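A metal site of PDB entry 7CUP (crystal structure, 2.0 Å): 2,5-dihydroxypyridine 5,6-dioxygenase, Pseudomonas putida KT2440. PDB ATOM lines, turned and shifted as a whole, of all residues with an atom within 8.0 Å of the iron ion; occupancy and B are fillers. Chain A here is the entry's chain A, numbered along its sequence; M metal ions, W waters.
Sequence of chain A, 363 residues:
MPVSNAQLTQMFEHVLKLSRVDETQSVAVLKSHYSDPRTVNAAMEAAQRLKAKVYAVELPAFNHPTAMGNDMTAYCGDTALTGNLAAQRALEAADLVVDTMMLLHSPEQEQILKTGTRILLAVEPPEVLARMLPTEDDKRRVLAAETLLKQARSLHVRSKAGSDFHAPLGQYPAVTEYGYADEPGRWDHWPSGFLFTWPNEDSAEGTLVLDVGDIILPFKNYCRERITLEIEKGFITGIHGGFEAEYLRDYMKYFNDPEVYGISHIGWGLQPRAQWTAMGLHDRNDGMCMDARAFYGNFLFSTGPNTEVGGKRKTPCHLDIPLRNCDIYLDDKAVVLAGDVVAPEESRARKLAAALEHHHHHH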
ATOM      1  N   THR A  73       5.536  13.135 -16.713  1.00  0.00           N
ATOM      2  CA  THR A  73       6.966  13.540 -16.531  1.00  0.00           C
ATOM      3  C   THR A  73       7.243  13.803 -15.050  1.00  0.00           C
ATOM      4  O   THR A  73       8.438  13.872 -14.690  1.00  0.00           O
ATOM      5  CB  THR A  73       7.336  14.794 -17.340  1.00  0.00           C
ATOM      6  OG1 THR A  73       6.754  15.948 -16.728  1.00  0.00           O
ATOM      7  CG2 THR A  73       6.911  14.663 -18.794  1.00  0.00           C
ATOM      8  N   CYS A  76       9.256   9.659 -12.251  1.00  0.00           N
ATOM      9  CA  CYS A  76      10.157   8.726 -13.000  1.00  0.00           C
ATOM     10  C   CYS A  76      10.385   7.486 -12.150  1.00  0.00           C
ATOM     11  O   CYS A  76      11.230   7.511 -11.253  1.00  0.00           O
ATOM     12  CB  CYS A  76      11.472   9.402 -13.352  1.00  0.00           C
ATOM     13  SG  CYS A  76      11.235  10.845 -14.402  1.00  0.00           S
ATOM     14  N   PHE A 194      15.383  20.883 -29.740  1.00  0.00           N
ATOM     15  CA  PHE A 194      16.340  21.351 -28.711  1.00  0.00           C
ATOM     16  C   PHE A 194      17.385  20.274 -28.418  1.00  0.00           C
ATOM     17  O   PHE A 194      17.372  19.167 -29.024  1.00  0.00           O
ATOM     18  CB  PHE A 194      15.591  21.795 -27.447  1.00  0.00           C
ATOM     19  CG  PHE A 194      14.805  20.729 -26.743  1.00  0.00           C
ATOM     20  CD1 PHE A 194      13.548  20.320 -27.211  1.00  0.00           C
ATOM     21  CD2 PHE A 194      15.274  20.164 -25.559  1.00  0.00           C
ATOM     22  CE1 PHE A 194      12.825  19.340 -26.548  1.00  0.00           C
ATOM     23  CE2 PHE A 194      14.522  19.197 -24.878  1.00  0.00           C
ATOM     24  CZ  PHE A 194      13.309  18.788 -25.388  1.00  0.00           C
ATOM     25  N   PHE A 196      20.602  19.002 -25.153  1.00  0.00           N
ATOM     26  CA  PHE A 196      21.068  19.059 -23.768  1.00  0.00           C
ATOM     27  C   PHE A 196      22.194  18.030 -23.546  1.00  0.00           C
ATOM     28  O   PHE A 196      22.352  17.123 -24.372  1.00  0.00           O
ATOM     29  CB  PHE A 196      19.896  18.801 -22.821  1.00  0.00           C
ATOM     30  CG  PHE A 196      19.079  17.575 -23.174  1.00  0.00           C
ATOM     31  CD1 PHE A 196      19.406  16.336 -22.647  1.00  0.00           C
ATOM     32  CD2 PHE A 196      17.995  17.673 -24.023  1.00  0.00           C
ATOM     33  CE1 PHE A 196      18.661  15.207 -22.972  1.00  0.00           C
ATOM     34  CE2 PHE A 196      17.243  16.553 -24.339  1.00  0.00           C
ATOM     35  CZ  PHE A 196      17.582  15.316 -23.829  1.00  0.00           C
ATOM     36  N   TRP A 198      24.484  16.521 -19.639  1.00  0.00           N
ATOM     37  CA  TRP A 198      24.523  16.488 -18.162  1.00  0.00           C
ATOM     38  C   TRP A 198      25.849  17.105 -17.726  1.00  0.00           C
ATOM     39  O   TRP A 198      26.839  16.988 -18.438  1.00  0.00           O
ATOM     40  CB  TRP A 198      24.352  15.041 -17.685  1.00  0.00           C
ATOM     41  CG  TRP A 198      23.012  14.471 -18.013  1.00  0.00           C
ATOM     42  CD1 TRP A 198      22.004  14.186 -17.127  1.00  0.00           C
ATOM     43  CD2 TRP A 198      22.530  14.073 -19.313  1.00  0.00           C
ATOM     44  NE1 TRP A 198      20.924  13.682 -17.792  1.00  0.00           N
ATOM     45  CE2 TRP A 198      21.221  13.592 -19.125  1.00  0.00           C
ATOM     46  CE3 TRP A 198      23.102  14.041 -20.591  1.00  0.00           C
ATOM     47  CZ2 TRP A 198      20.466  13.085 -20.178  1.00  0.00           C
ATOM     48  CZ3 TRP A 198      22.353  13.545 -21.638  1.00  0.00           C
ATOM     49  CH2 TRP A 198      21.047  13.095 -21.431  1.00  0.00           C
ATOM     50  N   LEU A 217       8.054  23.102 -14.765  1.00  0.00           N
ATOM     51  CA  LEU A 217       7.267  21.924 -15.189  1.00  0.00           C
ATOM     52  C   LEU A 217       7.568  20.791 -14.196  1.00  0.00           C
ATOM     53  O   LEU A 217       8.726  20.597 -13.864  1.00  0.00           O
ATOM     54  CB  LEU A 217       7.702  21.587 -16.622  1.00  0.00           C
ATOM     55  CG  LEU A 217       7.594  22.729 -17.624  1.00  0.00           C
ATOM     56  CD1 LEU A 217       8.110  22.287 -18.966  1.00  0.00           C
ATOM     57  CD2 LEU A 217       6.164  23.224 -17.758  1.00  0.00           C
ATOM     58  N   SER A 264      20.268  17.621 -13.400  1.00  0.00           N
ATOM     59  CA  SER A 264      20.261  16.628 -14.490  1.00  0.00           C
ATOM     60  C   SER A 264      20.634  17.351 -15.784  1.00  0.00           C
ATOM     61  O   SER A 264      21.746  17.862 -15.884  1.00  0.00           O
ATOM     62  CB  SER A 264      18.940  15.899 -14.558  1.00  0.00           C
ATOM     63  OG  SER A 264      18.955  14.808 -13.650  1.00  0.00           O
ATOM     64  N   HIS A 265      19.752  17.379 -16.784  1.00  0.00           N
ATOM     65  CA  HIS A 265      20.158  17.833 -18.132  1.00  0.00           C
ATOM     66  C   HIS A 265      20.150  19.355 -18.181  1.00  0.00           C
ATOM     67  O   HIS A 265      19.440  19.991 -17.367  1.00  0.00           O
ATOM     68  CB  HIS A 265      19.348  17.110 -19.219  1.00  0.00           C
ATOM     69  CG  HIS A 265      17.886  17.363 -19.189  1.00  0.00           C
ATOM     70  ND1 HIS A 265      17.315  18.489 -19.745  1.00  0.00           N
ATOM     71  CD2 HIS A 265      16.874  16.617 -18.696  1.00  0.00           C
ATOM     72  CE1 HIS A 265      16.010  18.448 -19.587  1.00  0.00           C
ATOM     73  NE2 HIS A 265      15.720  17.314 -18.938  1.00  0.00           N
ATOM     74  N   ILE A 266      20.970  19.917 -19.060  1.00  0.00           N
ATOM     75  CA  ILE A 266      21.200  21.376 -19.210  1.00  0.00           C
ATOM     76  C   ILE A 266      21.351  21.572 -20.701  1.00  0.00           C
ATOM     77  O   ILE A 266      21.999  20.727 -21.320  1.00  0.00           O
ATOM     78  CB  ILE A 266      22.432  21.800 -18.388  1.00  0.00           C
ATOM     79  CG1 ILE A 266      23.653  20.934 -18.666  1.00  0.00           C
ATOM     80  CG2 ILE A 266      22.116  21.784 -16.911  1.00  0.00           C
ATOM     81  CD1 ILE A 266      24.933  21.481 -18.064  1.00  0.00           C
ATOM     82  N   ARG A 293       9.571  23.741 -22.971  1.00  0.00           N
ATOM     83  CA  ARG A 293      10.896  23.071 -23.036  1.00  0.00           C
ATOM     84  C   ARG A 293      11.686  23.575 -24.253  1.00  0.00           C
ATOM     85  O   ARG A 293      12.923  23.602 -24.177  1.00  0.00           O
ATOM     86  CB  ARG A 293      10.783  21.544 -23.060  1.00  0.00           C
ATOM     87  CG  ARG A 293      10.180  20.936 -21.813  1.00  0.00           C
ATOM     88  CD  ARG A 293      10.137  19.435 -21.871  1.00  0.00           C
ATOM     89  NE  ARG A 293       9.709  18.935 -20.583  1.00  0.00           N
ATOM     90  CZ  ARG A 293       8.456  18.895 -20.154  1.00  0.00           C
ATOM     91  NH1 ARG A 293       7.466  19.329 -20.936  1.00  0.00           N
ATOM     92  NH2 ARG A 293       8.179  18.417 -18.941  1.00  0.00           N
ATOM     93  N   LEU A 300      17.313  25.440 -20.557  1.00  0.00           N
ATOM     94  CA  LEU A 300      16.483  24.405 -19.904  1.00  0.00           C
ATOM     95  C   LEU A 300      17.409  23.579 -19.041  1.00  0.00           C
ATOM     96  O   LEU A 300      18.319  22.954 -19.602  1.00  0.00           O
ATOM     97  CB  LEU A 300      15.813  23.528 -20.965  1.00  0.00           C
ATOM     98  CG  LEU A 300      14.923  22.420 -20.414  1.00  0.00           C
ATOM     99  CD1 LEU A 300      13.754  22.990 -19.625  1.00  0.00           C
ATOM    100  CD2 LEU A 300      14.439  21.530 -21.554  1.00  0.00           C
ATOM    101  N   PHE A 301      17.144  23.553 -17.752  1.00  0.00           N
ATOM    102  CA  PHE A 301      17.785  22.575 -16.854  1.00  0.00           C
ATOM    103  C   PHE A 301      16.704  21.712 -16.217  1.00  0.00           C
ATOM    104  O   PHE A 301      15.524  22.086 -16.229  1.00  0.00           O
ATOM    105  CB  PHE A 301      18.675  23.233 -15.806  1.00  0.00           C
ATOM    106  CG  PHE A 301      17.992  24.080 -14.781  1.00  0.00           C
ATOM    107  CD1 PHE A 301      17.531  25.352 -15.101  1.00  0.00           C
ATOM    108  CD2 PHE A 301      17.821  23.624 -13.478  1.00  0.00           C
ATOM    109  CE1 PHE A 301      16.914  26.141 -14.149  1.00  0.00           C
ATOM    110  CE2 PHE A 301      17.209  24.415 -12.534  1.00  0.00           C
ATOM    111  CZ  PHE A 301      16.758  25.669 -12.862  1.00  0.00           C
ATOM    112  N   SER A 302      17.161  20.613 -15.651  1.00  0.00           N
ATOM    113  CA  SER A 302      16.301  19.593 -15.030  1.00  0.00           C
ATOM    114  C   SER A 302      16.915  19.160 -13.687  1.00  0.00           C
ATOM    115  O   SER A 302      18.117  19.445 -13.450  1.00  0.00           O
ATOM    116  CB  SER A 302      16.116  18.440 -15.986  1.00  0.00           C
ATOM    117  OG  SER A 302      15.314  17.452 -15.368  1.00  0.00           O
ATOM    118  N   THR A 303      16.100  18.497 -12.870  1.00  0.00           N
ATOM    119  CA  THR A 303      16.484  18.006 -11.525  1.00  0.00           C
ATOM    120  C   THR A 303      16.085  16.531 -11.398  1.00  0.00           C
ATOM    121  O   THR A 303      15.165  16.102 -12.112  1.00  0.00           O
ATOM    122  CB  THR A 303      15.844  18.852 -10.420  1.00  0.00           C
ATOM    123  OG1 THR A 303      14.445  18.576 -10.376  1.00  0.00           O
ATOM    124  CG2 THR A 303      16.114  20.330 -10.612  1.00  0.00           C
ATOM    125  N   GLY A 304      16.765  15.827 -10.494  1.00  0.00           N
ATOM    126  CA  GLY A 304      16.420  14.456 -10.078  1.00  0.00           C
ATOM    127  C   GLY A 304      17.212  13.417 -10.871  1.00  0.00           C
ATOM    128  O   GLY A 304      18.438  13.482 -10.945  1.00  0.00           O
ATOM    129  N   PRO A 305      16.515  12.432 -11.473  1.00  0.00           N
ATOM    130  CA  PRO A 305      17.156  11.208 -11.956  1.00  0.00           C
ATOM    131  C   PRO A 305      18.093  11.457 -13.144  1.00  0.00           C
ATOM    132  O   PRO A 305      17.853  12.367 -13.917  1.00  0.00           O
ATOM    133  CB  PRO A 305      15.988  10.317 -12.407  1.00  0.00           C
ATOM    134  CG  PRO A 305      14.852  11.303 -12.705  1.00  0.00           C
ATOM    135  CD  PRO A 305      15.064  12.462 -11.753  1.00  0.00           C
ATOM    136  N   GLU A 308      19.299   7.379 -16.909  1.00  0.00           N
ATOM    137  CA  GLU A 308      19.109   7.268 -18.380  1.00  0.00           C
ATOM    138  C   GLU A 308      20.460   7.410 -19.107  1.00  0.00           C
ATOM    139  O   GLU A 308      20.539   6.926 -20.221  1.00  0.00           O
ATOM    140  CB  GLU A 308      18.107   8.303 -18.908  1.00  0.00           C
ATOM    141  CG  GLU A 308      18.582   9.732 -18.765  1.00  0.00           C
ATOM    142  CD  GLU A 308      17.472  10.775 -18.875  1.00  0.00           C
ATOM    143  OE1 GLU A 308      17.078  11.100 -20.005  1.00  0.00           O
ATOM    144  OE2 GLU A 308      17.008  11.239 -17.814  1.00  0.00           O
ATOM    145  N   HIS A 318      11.061  14.763 -10.658  1.00  0.00           N
ATOM    146  CA  HIS A 318      11.652  15.328 -11.895  1.00  0.00           C
ATOM    147  C   HIS A 318      11.047  16.713 -12.190  1.00  0.00           C
ATOM    148  O   HIS A 318       9.811  16.819 -12.356  1.00  0.00           O
ATOM    149  CB  HIS A 318      11.423  14.349 -13.030  1.00  0.00           C
ATOM    150  CG  HIS A 318      11.793  14.929 -14.347  1.00  0.00           C
ATOM    151  ND1 HIS A 318      10.860  15.232 -15.305  1.00  0.00           N
ATOM    152  CD2 HIS A 318      12.978  15.323 -14.820  1.00  0.00           C
ATOM    153  CE1 HIS A 318      11.445  15.775 -16.340  1.00  0.00           C
ATOM    154  NE2 HIS A 318      12.744  15.835 -16.068  1.00  0.00           N
ATOM    155  N   LEU A 319      11.903  17.732 -12.309  1.00  0.00           N
ATOM    156  CA  LEU A 319      11.497  19.098 -12.749  1.00  0.00           C
ATOM    157  C   LEU A 319      12.261  19.494 -14.000  1.00  0.00           C
ATOM    158  O   LEU A 319      13.445  19.132 -14.118  1.00  0.00           O
ATOM    159  CB  LEU A 319      11.767  20.115 -11.629  1.00  0.00           C
ATOM    160  CG  LEU A 319      11.126  19.796 -10.292  1.00  0.00           C
ATOM    161  CD1 LEU A 319      11.527  20.851  -9.259  1.00  0.00           C
ATOM    162  CD2 LEU A 319       9.601  19.698 -10.384  1.00  0.00           C
ATOM    163  N   ASP A 320      11.554  20.122 -14.948  1.00  0.00           N
ATOM    164  CA  ASP A 320      12.111  20.822 -16.127  1.00  0.00           C
ATOM    165  C   ASP A 320      11.832  22.297 -15.931  1.00  0.00           C
ATOM    166  O   ASP A 320      10.654  22.661 -15.635  1.00  0.00           O
ATOM    167  CB  ASP A 320      11.526  20.310 -17.442  1.00  0.00           C
ATOM    168  CG  ASP A 320      12.116  18.974 -17.842  1.00  0.00           C
ATOM    169  OD1 ASP A 320      13.216  18.695 -17.391  1.00  0.00           O
ATOM    170  OD2 ASP A 320      11.452  18.220 -18.572  1.00  0.00           O
ATOM    171  N   ILE A 321      12.868  23.109 -16.065  1.00  0.00           N
ATOM    172  CA  ILE A 321      12.803  24.567 -15.745  1.00  0.00           C
ATOM    173  C   ILE A 321      13.494  25.336 -16.868  1.00  0.00           C
ATOM    174  O   ILE A 321      14.724  25.372 -16.907  1.00  0.00           O
ATOM    175  CB  ILE A 321      13.452  24.847 -14.382  1.00  0.00           C
ATOM    176  CG1 ILE A 321      12.763  24.047 -13.286  1.00  0.00           C
ATOM    177  CG2 ILE A 321      13.434  26.346 -14.121  1.00  0.00           C
ATOM    178  CD1 ILE A 321      13.438  24.138 -11.920  1.00  0.00           C
HETATM  179 FE    FE M   1      14.340  16.695 -17.316  1.00  0.00          FE
HETATM  180  O   HOH W   1      13.063  15.944 -19.094  1.00  0.00           O
HETATM  181  O   HOH W   2      15.286  14.666 -16.582  1.00  0.00           O
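The backbone carbonyl oxygen of Thr 73 is in hydrogen-bond range of a ring nitrogen (ND1) of His 318 (2.8 Å). OD2 of Asp 320 lies within salt-bridge range of NE of Arg 293 (2.8 Å). The backbone carbonyl oxygen (O) of Asp 320 is in hydrogen-bond range of the backbone NH (N) of Leu 217 (2.8 Å). O of Leu 319 sits close to OG of Ser 302 (2.8 Å). O of Ser 302 lies within hydrogen-bond range of N of Ser 264, 2.8 Å away.
Within 4 Å of the iron ion: His 265, Ser 302, His 318 and Asp 320.
The iron ion is bound by a ring nitrogen (NE2) of His 318, a ring nitrogen (NE2) of His 265, the side-chain carboxylate of Asp 320, the side-chain hydroxyl of Ser 302, water W1 and water W2. The iron ion has six donor atoms within binding distance.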
